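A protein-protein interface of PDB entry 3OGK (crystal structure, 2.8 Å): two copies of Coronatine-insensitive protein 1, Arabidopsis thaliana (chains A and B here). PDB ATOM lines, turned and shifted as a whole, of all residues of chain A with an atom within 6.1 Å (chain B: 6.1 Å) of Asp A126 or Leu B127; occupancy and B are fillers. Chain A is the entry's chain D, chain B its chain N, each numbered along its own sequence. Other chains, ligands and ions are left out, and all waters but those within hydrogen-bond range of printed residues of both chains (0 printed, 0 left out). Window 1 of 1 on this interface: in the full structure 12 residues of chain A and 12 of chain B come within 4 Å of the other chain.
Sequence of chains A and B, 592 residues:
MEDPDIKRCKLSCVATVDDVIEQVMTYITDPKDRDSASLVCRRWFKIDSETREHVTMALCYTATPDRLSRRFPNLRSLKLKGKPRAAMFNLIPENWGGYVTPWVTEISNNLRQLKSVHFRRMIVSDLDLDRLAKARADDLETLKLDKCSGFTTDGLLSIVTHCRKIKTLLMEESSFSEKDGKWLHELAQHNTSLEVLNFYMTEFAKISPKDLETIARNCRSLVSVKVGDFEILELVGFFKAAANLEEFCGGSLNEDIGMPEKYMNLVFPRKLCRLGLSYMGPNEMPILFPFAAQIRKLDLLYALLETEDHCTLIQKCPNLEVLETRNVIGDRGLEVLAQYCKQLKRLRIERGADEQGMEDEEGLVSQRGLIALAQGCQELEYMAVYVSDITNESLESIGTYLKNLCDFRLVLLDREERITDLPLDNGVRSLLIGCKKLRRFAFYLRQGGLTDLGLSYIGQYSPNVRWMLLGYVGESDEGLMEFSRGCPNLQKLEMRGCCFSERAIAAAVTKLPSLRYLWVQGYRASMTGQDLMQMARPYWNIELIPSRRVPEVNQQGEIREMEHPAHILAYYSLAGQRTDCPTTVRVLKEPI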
ATOM      1  N   VAL A 124     -25.370  -6.065  12.401  1.00  0.00           N
ATOM      2  CA  VAL A 124     -24.003  -5.799  12.025  1.00  0.00           C
ATOM      3  C   VAL A 124     -23.150  -5.850  13.289  1.00  0.00           C
ATOM      4  O   VAL A 124     -23.408  -5.100  14.200  1.00  0.00           O
ATOM      5  CB  VAL A 124     -23.863  -4.394  11.446  1.00  0.00           C
ATOM      6  CG1 VAL A 124     -22.411  -4.121  11.099  1.00  0.00           C
ATOM      7  CG2 VAL A 124     -24.747  -4.215  10.242  1.00  0.00           C
ATOM      8  N   SER A 125     -22.136  -6.714  13.348  1.00  0.00           N
ATOM      9  CA  SER A 125     -21.239  -6.769  14.496  1.00  0.00           C
ATOM     10  C   SER A 125     -19.931  -6.002  14.305  1.00  0.00           C
ATOM     11  O   SER A 125     -19.624  -5.525  13.217  1.00  0.00           O
ATOM     12  CB  SER A 125     -20.903  -8.200  14.835  1.00  0.00           C
ATOM     13  OG  SER A 125     -19.907  -8.720  13.967  1.00  0.00           O
ATOM     14  N   ASP A 126     -19.153  -5.880  15.379  1.00  0.00           N
ATOM     15  CA  ASP A 126     -17.908  -5.155  15.287  1.00  0.00           C
ATOM     16  C   ASP A 126     -16.955  -5.934  14.391  1.00  0.00           C
ATOM     17  O   ASP A 126     -16.171  -5.381  13.628  1.00  0.00           O
ATOM     18  CB  ASP A 126     -17.291  -4.997  16.655  1.00  0.00           C
ATOM     19  CG  ASP A 126     -17.783  -3.747  17.399  1.00  0.00           C
ATOM     20  OD1 ASP A 126     -18.431  -2.882  16.763  1.00  0.00           O
ATOM     21  OD2 ASP A 126     -17.501  -3.644  18.635  1.00  0.00           O
ATOM     22  N   LEU A 127     -17.015  -7.242  14.492  1.00  0.00           N
ATOM     23  CA  LEU A 127     -16.132  -8.054  13.688  1.00  0.00           C
ATOM     24  C   LEU A 127     -16.479  -7.785  12.238  1.00  0.00           C
ATOM     25  O   LEU A 127     -15.613  -7.501  11.392  1.00  0.00           O
ATOM     26  CB  LEU A 127     -16.312  -9.534  13.981  1.00  0.00           C
ATOM     27  CG  LEU A 127     -15.384 -10.493  13.247  1.00  0.00           C
ATOM     28  CD1 LEU A 127     -13.946 -10.101  13.372  1.00  0.00           C
ATOM     29  CD2 LEU A 127     -15.581 -11.882  13.830  1.00  0.00           C
ATOM     30  N   ASP A 128     -17.757  -7.836  11.924  1.00  0.00           N
ATOM     31  CA  ASP A 128     -18.024  -7.677  10.515  1.00  0.00           C
ATOM     32  C   ASP A 128     -17.710  -6.251  10.011  1.00  0.00           C
ATOM     33  O   ASP A 128     -17.224  -6.102   8.900  1.00  0.00           O
ATOM     34  CB  ASP A 128     -19.301  -8.404   9.998  1.00  0.00           C
ATOM     35  CG  ASP A 128     -20.482  -8.233  10.886  1.00  0.00           C
ATOM     36  OD1 ASP A 128     -21.319  -9.161  10.991  1.00  0.00           O
ATOM     37  OD2 ASP A 128     -20.593  -7.150  11.478  1.00  0.00           O
ATOM     38  N   LEU A 129     -17.829  -5.211  10.833  1.00  0.00           N
ATOM     39  CA  LEU A 129     -17.297  -3.952  10.296  1.00  0.00           C
ATOM     40  C   LEU A 129     -15.812  -3.726  10.339  1.00  0.00           C
ATOM     41  O   LEU A 129     -15.291  -3.001   9.514  1.00  0.00           O
ATOM     42  CB  LEU A 129     -18.140  -2.682  10.479  1.00  0.00           C
ATOM     43  CG  LEU A 129     -18.760  -1.918  11.610  1.00  0.00           C
ATOM     44  CD1 LEU A 129     -20.034  -1.374  11.037  1.00  0.00           C
ATOM     45  CD2 LEU A 129     -19.074  -2.825  12.713  1.00  0.00           C
ATOM     46  N   ASP A 130     -15.105  -4.412  11.219  1.00  0.00           N
ATOM     47  CA  ASP A 130     -13.652  -4.403  11.134  1.00  0.00           C
ATOM     48  C   ASP A 130     -13.179  -5.099   9.824  1.00  0.00           C
ATOM     49  O   ASP A 130     -12.275  -4.629   9.139  1.00  0.00           O
ATOM     50  CB  ASP A 130     -13.048  -5.087  12.350  1.00  0.00           C
ATOM     51  CG  ASP A 130     -11.535  -4.979  12.378  1.00  0.00           C
ATOM     52  OD1 ASP A 130     -11.042  -3.834  12.518  1.00  0.00           O
ATOM     53  OD2 ASP A 130     -10.845  -6.030  12.261  1.00  0.00           O
ATOM     54  N   ARG A 131     -13.818  -6.205   9.459  1.00  0.00           N
ATOM     55  CA  ARG A 131     -13.476  -6.862   8.216  1.00  0.00           C
ATOM     56  C   ARG A 131     -13.772  -6.020   6.979  1.00  0.00           C
ATOM     57  O   ARG A 131     -12.978  -5.984   6.040  1.00  0.00           O
ATOM     58  CB  ARG A 131     -14.192  -8.178   8.095  1.00  0.00           C
ATOM     59  CG  ARG A 131     -13.654  -9.284   8.971  1.00  0.00           C
ATOM     60  CD  ARG A 131     -14.592 -10.463   8.813  1.00  0.00           C
ATOM     61  NE  ARG A 131     -14.250 -11.616   9.621  1.00  0.00           N
ATOM     62  CZ  ARG A 131     -15.127 -12.572   9.924  1.00  0.00           C
ATOM     63  NH1 ARG A 131     -16.382 -12.463   9.490  1.00  0.00           N
ATOM     64  NH2 ARG A 131     -14.765 -13.625  10.666  1.00  0.00           N
ATOM     65  N   GLY A 150     -26.351  -4.291  16.624  1.00  0.00           N
ATOM     66  CA  GLY A 150     -25.392  -5.343  16.918  1.00  0.00           C
ATOM     67  C   GLY A 150     -23.933  -4.958  17.022  1.00  0.00           C
ATOM     68  O   GLY A 150     -23.075  -5.809  17.270  1.00  0.00           O
ATOM     69  N   PHE A 151     -23.636  -3.682  16.828  1.00  0.00           N
ATOM     70  CA  PHE A 151     -22.254  -3.212  16.835  1.00  0.00           C
ATOM     71  C   PHE A 151     -21.982  -2.257  17.986  1.00  0.00           C
ATOM     72  O   PHE A 151     -22.832  -2.091  18.862  1.00  0.00           O
ATOM     73  CB  PHE A 151     -21.876  -2.563  15.499  1.00  0.00           C
ATOM     74  CG  PHE A 151     -22.763  -1.430  15.081  1.00  0.00           C
ATOM     75  CD1 PHE A 151     -22.374  -0.131  15.269  1.00  0.00           C
ATOM     76  CD2 PHE A 151     -23.970  -1.667  14.454  1.00  0.00           C
ATOM     77  CE1 PHE A 151     -23.182   0.915  14.855  1.00  0.00           C
ATOM     78  CE2 PHE A 151     -24.793  -0.614  14.044  1.00  0.00           C
ATOM     79  CZ  PHE A 151     -24.399   0.666  14.241  1.00  0.00           C
ATOM     80  N   THR A 152     -20.788  -1.654  17.984  1.00  0.00           N
ATOM     81  CA  THR A 152     -20.408  -0.689  19.002  1.00  0.00           C
ATOM     82  C   THR A 152     -19.482   0.320  18.405  1.00  0.00           C
ATOM     83  O   THR A 152     -19.121   0.219  17.253  1.00  0.00           O
ATOM     84  CB  THR A 152     -19.619  -1.311  20.139  1.00  0.00           C
ATOM     85  OG1 THR A 152     -18.247  -1.358  19.773  1.00  0.00           O
ATOM     86  CG2 THR A 152     -20.111  -2.717  20.450  1.00  0.00           C
ATOM     87  N   THR A 153     -19.088   1.302  19.206  1.00  0.00           N
ATOM     88  CA  THR A 153     -18.211   2.370  18.734  1.00  0.00           C
ATOM     89  C   THR A 153     -16.852   1.868  18.283  1.00  0.00           C
ATOM     90  O   THR A 153     -16.167   2.553  17.540  1.00  0.00           O
ATOM     91  CB  THR A 153     -18.055   3.453  19.779  1.00  0.00           C
ATOM     92  OG1 THR A 153     -17.654   2.858  21.017  1.00  0.00           O
ATOM     93  CG2 THR A 153     -19.357   4.126  20.006  1.00  0.00           C
ATOM     94  N   ASP A 154     -16.486   0.656  18.688  1.00  0.00           N
ATOM     95  CA  ASP A 154     -15.260   0.012  18.180  1.00  0.00           C
ATOM     96  C   ASP A 154     -15.342  -0.247  16.652  1.00  0.00           C
ATOM     97  O   ASP A 154     -14.363  -0.061  15.895  1.00  0.00           O
ATOM     98  CB  ASP A 154     -14.956  -1.317  18.914  1.00  0.00           C
ATOM     99  CG  ASP A 154     -14.560  -1.126  20.378  1.00  0.00           C
ATOM    100  OD1 ASP A 154     -14.192   0.009  20.804  1.00  0.00           O
ATOM    101  OD2 ASP A 154     -14.634  -2.147  21.097  1.00  0.00           O
ATOM    102  N   GLY A 155     -16.521  -0.685  16.215  1.00  0.00           N
ATOM    103  CA  GLY A 155     -16.774  -0.856  14.810  1.00  0.00           C
ATOM    104  C   GLY A 155     -16.649   0.466  14.091  1.00  0.00           C
ATOM    105  O   GLY A 155     -15.954   0.567  13.088  1.00  0.00           O
ATOM    106  N   LEU A 156     -17.324   1.493  14.598  1.00  0.00           N
ATOM    107  CA  LEU A 156     -17.264   2.815  13.978  1.00  0.00           C
ATOM    108  C   LEU A 156     -15.840   3.303  13.856  1.00  0.00           C
ATOM    109  O   LEU A 156     -15.441   3.832  12.832  1.00  0.00           O
ATOM    110  CB  LEU A 156     -18.087   3.833  14.747  1.00  0.00           C
ATOM    111  CG  LEU A 156     -19.588   3.550  14.790  1.00  0.00           C
ATOM    112  CD1 LEU A 156     -20.188   4.784  15.369  1.00  0.00           C
ATOM    113  CD2 LEU A 156     -20.206   3.282  13.413  1.00  0.00           C
ATOM    114  N   SER A 158     -13.201   1.575  13.746  1.00  0.00           N
ATOM    115  CA  SER A 158     -12.471   0.770  12.786  1.00  0.00           C
ATOM    116  C   SER A 158     -12.712   1.296  11.382  1.00  0.00           C
ATOM    117  O   SER A 158     -11.755   1.471  10.637  1.00  0.00           O
ATOM    118  CB  SER A 158     -12.805  -0.699  12.915  1.00  0.00           C
ATOM    119  OG  SER A 158     -12.047  -1.425  11.979  1.00  0.00           O
ATOM    120  N   LYS A 179     -19.282   2.992  23.798  1.00  0.00           N
ATOM    121  CA  LYS A 179     -18.215   2.980  24.784  1.00  0.00           C
ATOM    122  C   LYS A 179     -17.400   4.290  24.831  1.00  0.00           C
ATOM    123  O   LYS A 179     -16.821   4.617  25.852  1.00  0.00           O
ATOM    124  CB  LYS A 179     -17.274   1.803  24.491  1.00  0.00           C
ATOM    125  CG  LYS A 179     -17.943   0.432  24.488  1.00  0.00           C
ATOM    126  CD  LYS A 179     -17.346  -0.476  23.400  1.00  0.00           C
ATOM    127  CE  LYS A 179     -16.025  -1.045  23.709  1.00  0.00           C
ATOM    128  NZ  LYS A 179     -16.030  -2.419  23.158  1.00  0.00           N
ATOM    129  N   VAL B 104      -8.205  -7.272  25.845  1.00  0.00           N
ATOM    130  CA  VAL B 104      -7.615  -8.126  24.837  1.00  0.00           C
ATOM    131  C   VAL B 104      -6.654  -7.322  23.998  1.00  0.00           C
ATOM    132  O   VAL B 104      -5.665  -7.883  23.551  1.00  0.00           O
ATOM    133  CB  VAL B 104      -8.563  -8.990  23.992  1.00  0.00           C
ATOM    134  CG1 VAL B 104      -9.847  -9.217  24.681  1.00  0.00           C
ATOM    135  CG2 VAL B 104      -8.738  -8.431  22.588  1.00  0.00           C
ATOM    136  N   SER B 125     -17.115  -9.238  22.575  1.00  0.00           N
ATOM    137  CA  SER B 125     -17.595  -9.220  21.173  1.00  0.00           C
ATOM    138  C   SER B 125     -16.866 -10.194  20.235  1.00  0.00           C
ATOM    139  O   SER B 125     -15.831 -10.707  20.580  1.00  0.00           O
ATOM    140  CB  SER B 125     -17.546  -7.802  20.595  1.00  0.00           C
ATOM    141  OG  SER B 125     -16.239  -7.360  20.261  1.00  0.00           O
ATOM    142  N   ASP B 126     -17.384 -10.424  19.039  1.00  0.00           N
ATOM    143  CA  ASP B 126     -16.661 -11.232  18.073  1.00  0.00           C
ATOM    144  C   ASP B 126     -15.336 -10.604  17.712  1.00  0.00           C
ATOM    145  O   ASP B 126     -14.366 -11.302  17.480  1.00  0.00           O
ATOM    146  CB  ASP B 126     -17.466 -11.355  16.808  1.00  0.00           C
ATOM    147  CG  ASP B 126     -18.540 -12.383  16.919  1.00  0.00           C
ATOM    148  OD1 ASP B 126     -18.461 -13.202  17.860  1.00  0.00           O
ATOM    149  OD2 ASP B 126     -19.440 -12.389  16.049  1.00  0.00           O
ATOM    150  N   LEU B 127     -15.293  -9.282  17.657  1.00  0.00           N
ATOM    151  CA  LEU B 127     -14.073  -8.612  17.296  1.00  0.00           C
ATOM    152  C   LEU B 127     -13.077  -8.932  18.360  1.00  0.00           C
ATOM    153  O   LEU B 127     -11.906  -9.233  18.080  1.00  0.00           O
ATOM    154  CB  LEU B 127     -14.243  -7.104  17.237  1.00  0.00           C
ATOM    155  CG  LEU B 127     -12.993  -6.339  16.745  1.00  0.00           C
ATOM    156  CD1 LEU B 127     -12.388  -6.925  15.427  1.00  0.00           C
ATOM    157  CD2 LEU B 127     -13.332  -4.863  16.553  1.00  0.00           C
ATOM    158  N   ASP B 128     -13.504  -8.862  19.606  1.00  0.00           N
ATOM    159  CA  ASP B 128     -12.462  -9.011  20.599  1.00  0.00           C
ATOM    160  C   ASP B 128     -12.050 -10.471  20.732  1.00  0.00           C
ATOM    161  O   ASP B 128     -10.876 -10.754  21.005  1.00  0.00           O
ATOM    162  CB  ASP B 128     -12.623  -8.172  21.909  1.00  0.00           C
ATOM    163  CG  ASP B 128     -14.015  -8.153  22.421  1.00  0.00           C
ATOM    164  OD1 ASP B 128     -14.423  -7.154  23.058  1.00  0.00           O
ATOM    165  OD2 ASP B 128     -14.715  -9.157  22.194  1.00  0.00           O
ATOM    166  N   LEU B 129     -12.928 -11.418  20.427  1.00  0.00           N
ATOM    167  CA  LEU B 129     -12.334 -12.748  20.366  1.00  0.00           C
ATOM    168  C   LEU B 129     -11.555 -13.127  19.106  1.00  0.00           C
ATOM    169  O   LEU B 129     -10.574 -13.849  19.194  1.00  0.00           O
ATOM    170  CB  LEU B 129     -13.107 -13.890  21.052  1.00  0.00           C
ATOM    171  CG  LEU B 129     -14.461 -14.518  20.954  1.00  0.00           C
ATOM    172  CD1 LEU B 129     -14.726 -14.908  22.410  1.00  0.00           C
ATOM    173  CD2 LEU B 129     -15.480 -13.562  20.470  1.00  0.00           C
ATOM    174  N   ASP B 130     -11.914 -12.587  17.958  1.00  0.00           N
ATOM    175  CA  ASP B 130     -11.038 -12.727  16.794  1.00  0.00           C
ATOM    176  C   ASP B 130      -9.623 -12.197  17.100  1.00  0.00           C
ATOM    177  O   ASP B 130      -8.629 -12.838  16.739  1.00  0.00           O
ATOM    178  CB  ASP B 130     -11.625 -11.991  15.583  1.00  0.00           C
ATOM    179  CG  ASP B 130     -10.868 -12.268  14.314  1.00  0.00           C
ATOM    180  OD1 ASP B 130     -10.932 -13.425  13.859  1.00  0.00           O
ATOM    181  OD2 ASP B 130     -10.236 -11.334  13.771  1.00  0.00           O
ATOM    182  N   ARG B 131      -9.525 -11.049  17.771  1.00  0.00           N
ATOM    183  CA  ARG B 131      -8.203 -10.494  18.110  1.00  0.00           C
ATOM    184  C   ARG B 131      -7.420 -11.376  19.085  1.00  0.00           C
ATOM    185  O   ARG B 131      -6.206 -11.470  18.973  1.00  0.00           O
ATOM    186  CB  ARG B 131      -8.305  -9.118  18.727  1.00  0.00           C
ATOM    187  CG  ARG B 131      -8.635  -8.026  17.763  1.00  0.00           C
ATOM    188  CD  ARG B 131      -8.922  -6.794  18.535  1.00  0.00           C
ATOM    189  NE  ARG B 131      -9.220  -5.643  17.711  1.00  0.00           N
ATOM    190  CZ  ARG B 131      -9.809  -4.557  18.193  1.00  0.00           C
ATOM    191  NH1 ARG B 131     -10.160  -4.530  19.481  1.00  0.00           N
ATOM    192  NH2 ARG B 131     -10.050  -3.512  17.401  1.00  0.00           N
ATOM    193  N   LEU B 132      -8.111 -11.984  20.056  1.00  0.00           N
ATOM    194  CA  LEU B 132      -7.489 -12.838  21.065  1.00  0.00           C
ATOM    195  C   LEU B 132      -6.981 -14.060  20.380  1.00  0.00           C
ATOM    196  O   LEU B 132      -5.857 -14.479  20.609  1.00  0.00           O
ATOM    197  CB  LEU B 132      -8.531 -13.327  22.054  1.00  0.00           C
ATOM    198  CG  LEU B 132      -8.128 -13.531  23.513  1.00  0.00           C
ATOM    199  CD1 LEU B 132      -8.860 -14.758  24.060  1.00  0.00           C
ATOM    200  CD2 LEU B 132      -6.668 -13.668  23.682  1.00  0.00           C
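Of the printed residues of chain B, Asp A126 touches Leu B127.
Of the printed residues of chain B, Leu A127 touches Asp B126 (3.6 Å), Leu B127 (3.8 Å) and Asp B130 (3.7 Å).
Of the printed residues of chain B, Asp A130 touches Leu B127.
Of the printed residues of chain A, Asp B126 touches Leu A127.
Printed residues of chain A within 4 Å of Asp B130: Leu A127.
The nearest residue of chain A that does not touch Leu B127 is Asp A154 (4.6 Å).
Asp A126 touches Leu B127 (CB to CB, 3.8 Å).
CB of Asp B126 touches CB of Leu A127, at 3.6 Å.
Leu A127 touches Leu B127 (CB to N, 3.8 Å).
Asp B130 touches Leu A127 (CB to CD1, 3.7 Å).
CD1 of Leu B127 touches OD2 of Asp A130 (3.6 Å).
The side-chain hydroxyl (OG) of Ser A125 sits close to the backbone NH (N) of Leu A127, 3.3 Å away.
The side-chain carboxylate (OD2) of Asp A126 sits at hydrogen-bond distance from the side-chain hydroxyl (OG1) of Thr A152, 2.7 Å away.
The side-chain carboxylate (OD1) of Asp A126 sits at hydrogen-bond distance from the backbone NH (N) of Gly A155 (3.0 Å).
The side-chain hydroxyl (OG) of Ser A158 lies within hydrogen-bond range of the side-chain carboxylate (OD1) of Asp A130, at 2.7 Å.
The side-chain hydroxyl (OG) of Ser B125 sits close to the backbone NH (N) of Leu B127 (3.4 Å).
Hydrophobic or aromatic side chains of chain A within 4 Å of the printed part of chain B: Leu A127.
Of the 9 printed residues of chain B, 3 touch a printed residue of chain A.
Printed residues of chain B that touch a printed residue of chain A: Asp B126, Leu B127 and Asp B130.
Hydrophobic or aromatic side chains of chain B within 4 Å of the printed part of chain A: Leu B127.
Among the printed residues, 5 pairs touch across the chains.
Asp A126 touches Leu B127, and with the chains exchanged Leu A127 touches Asp B126.
Leu A127 touches its own counterpart, Leu B127.
Leu A127 touches Asp B130, and with the chains exchanged Asp A130 touches Leu B127.
Positions printed for both chains: 125, 126, 127, 128, 129, 130 and 131.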
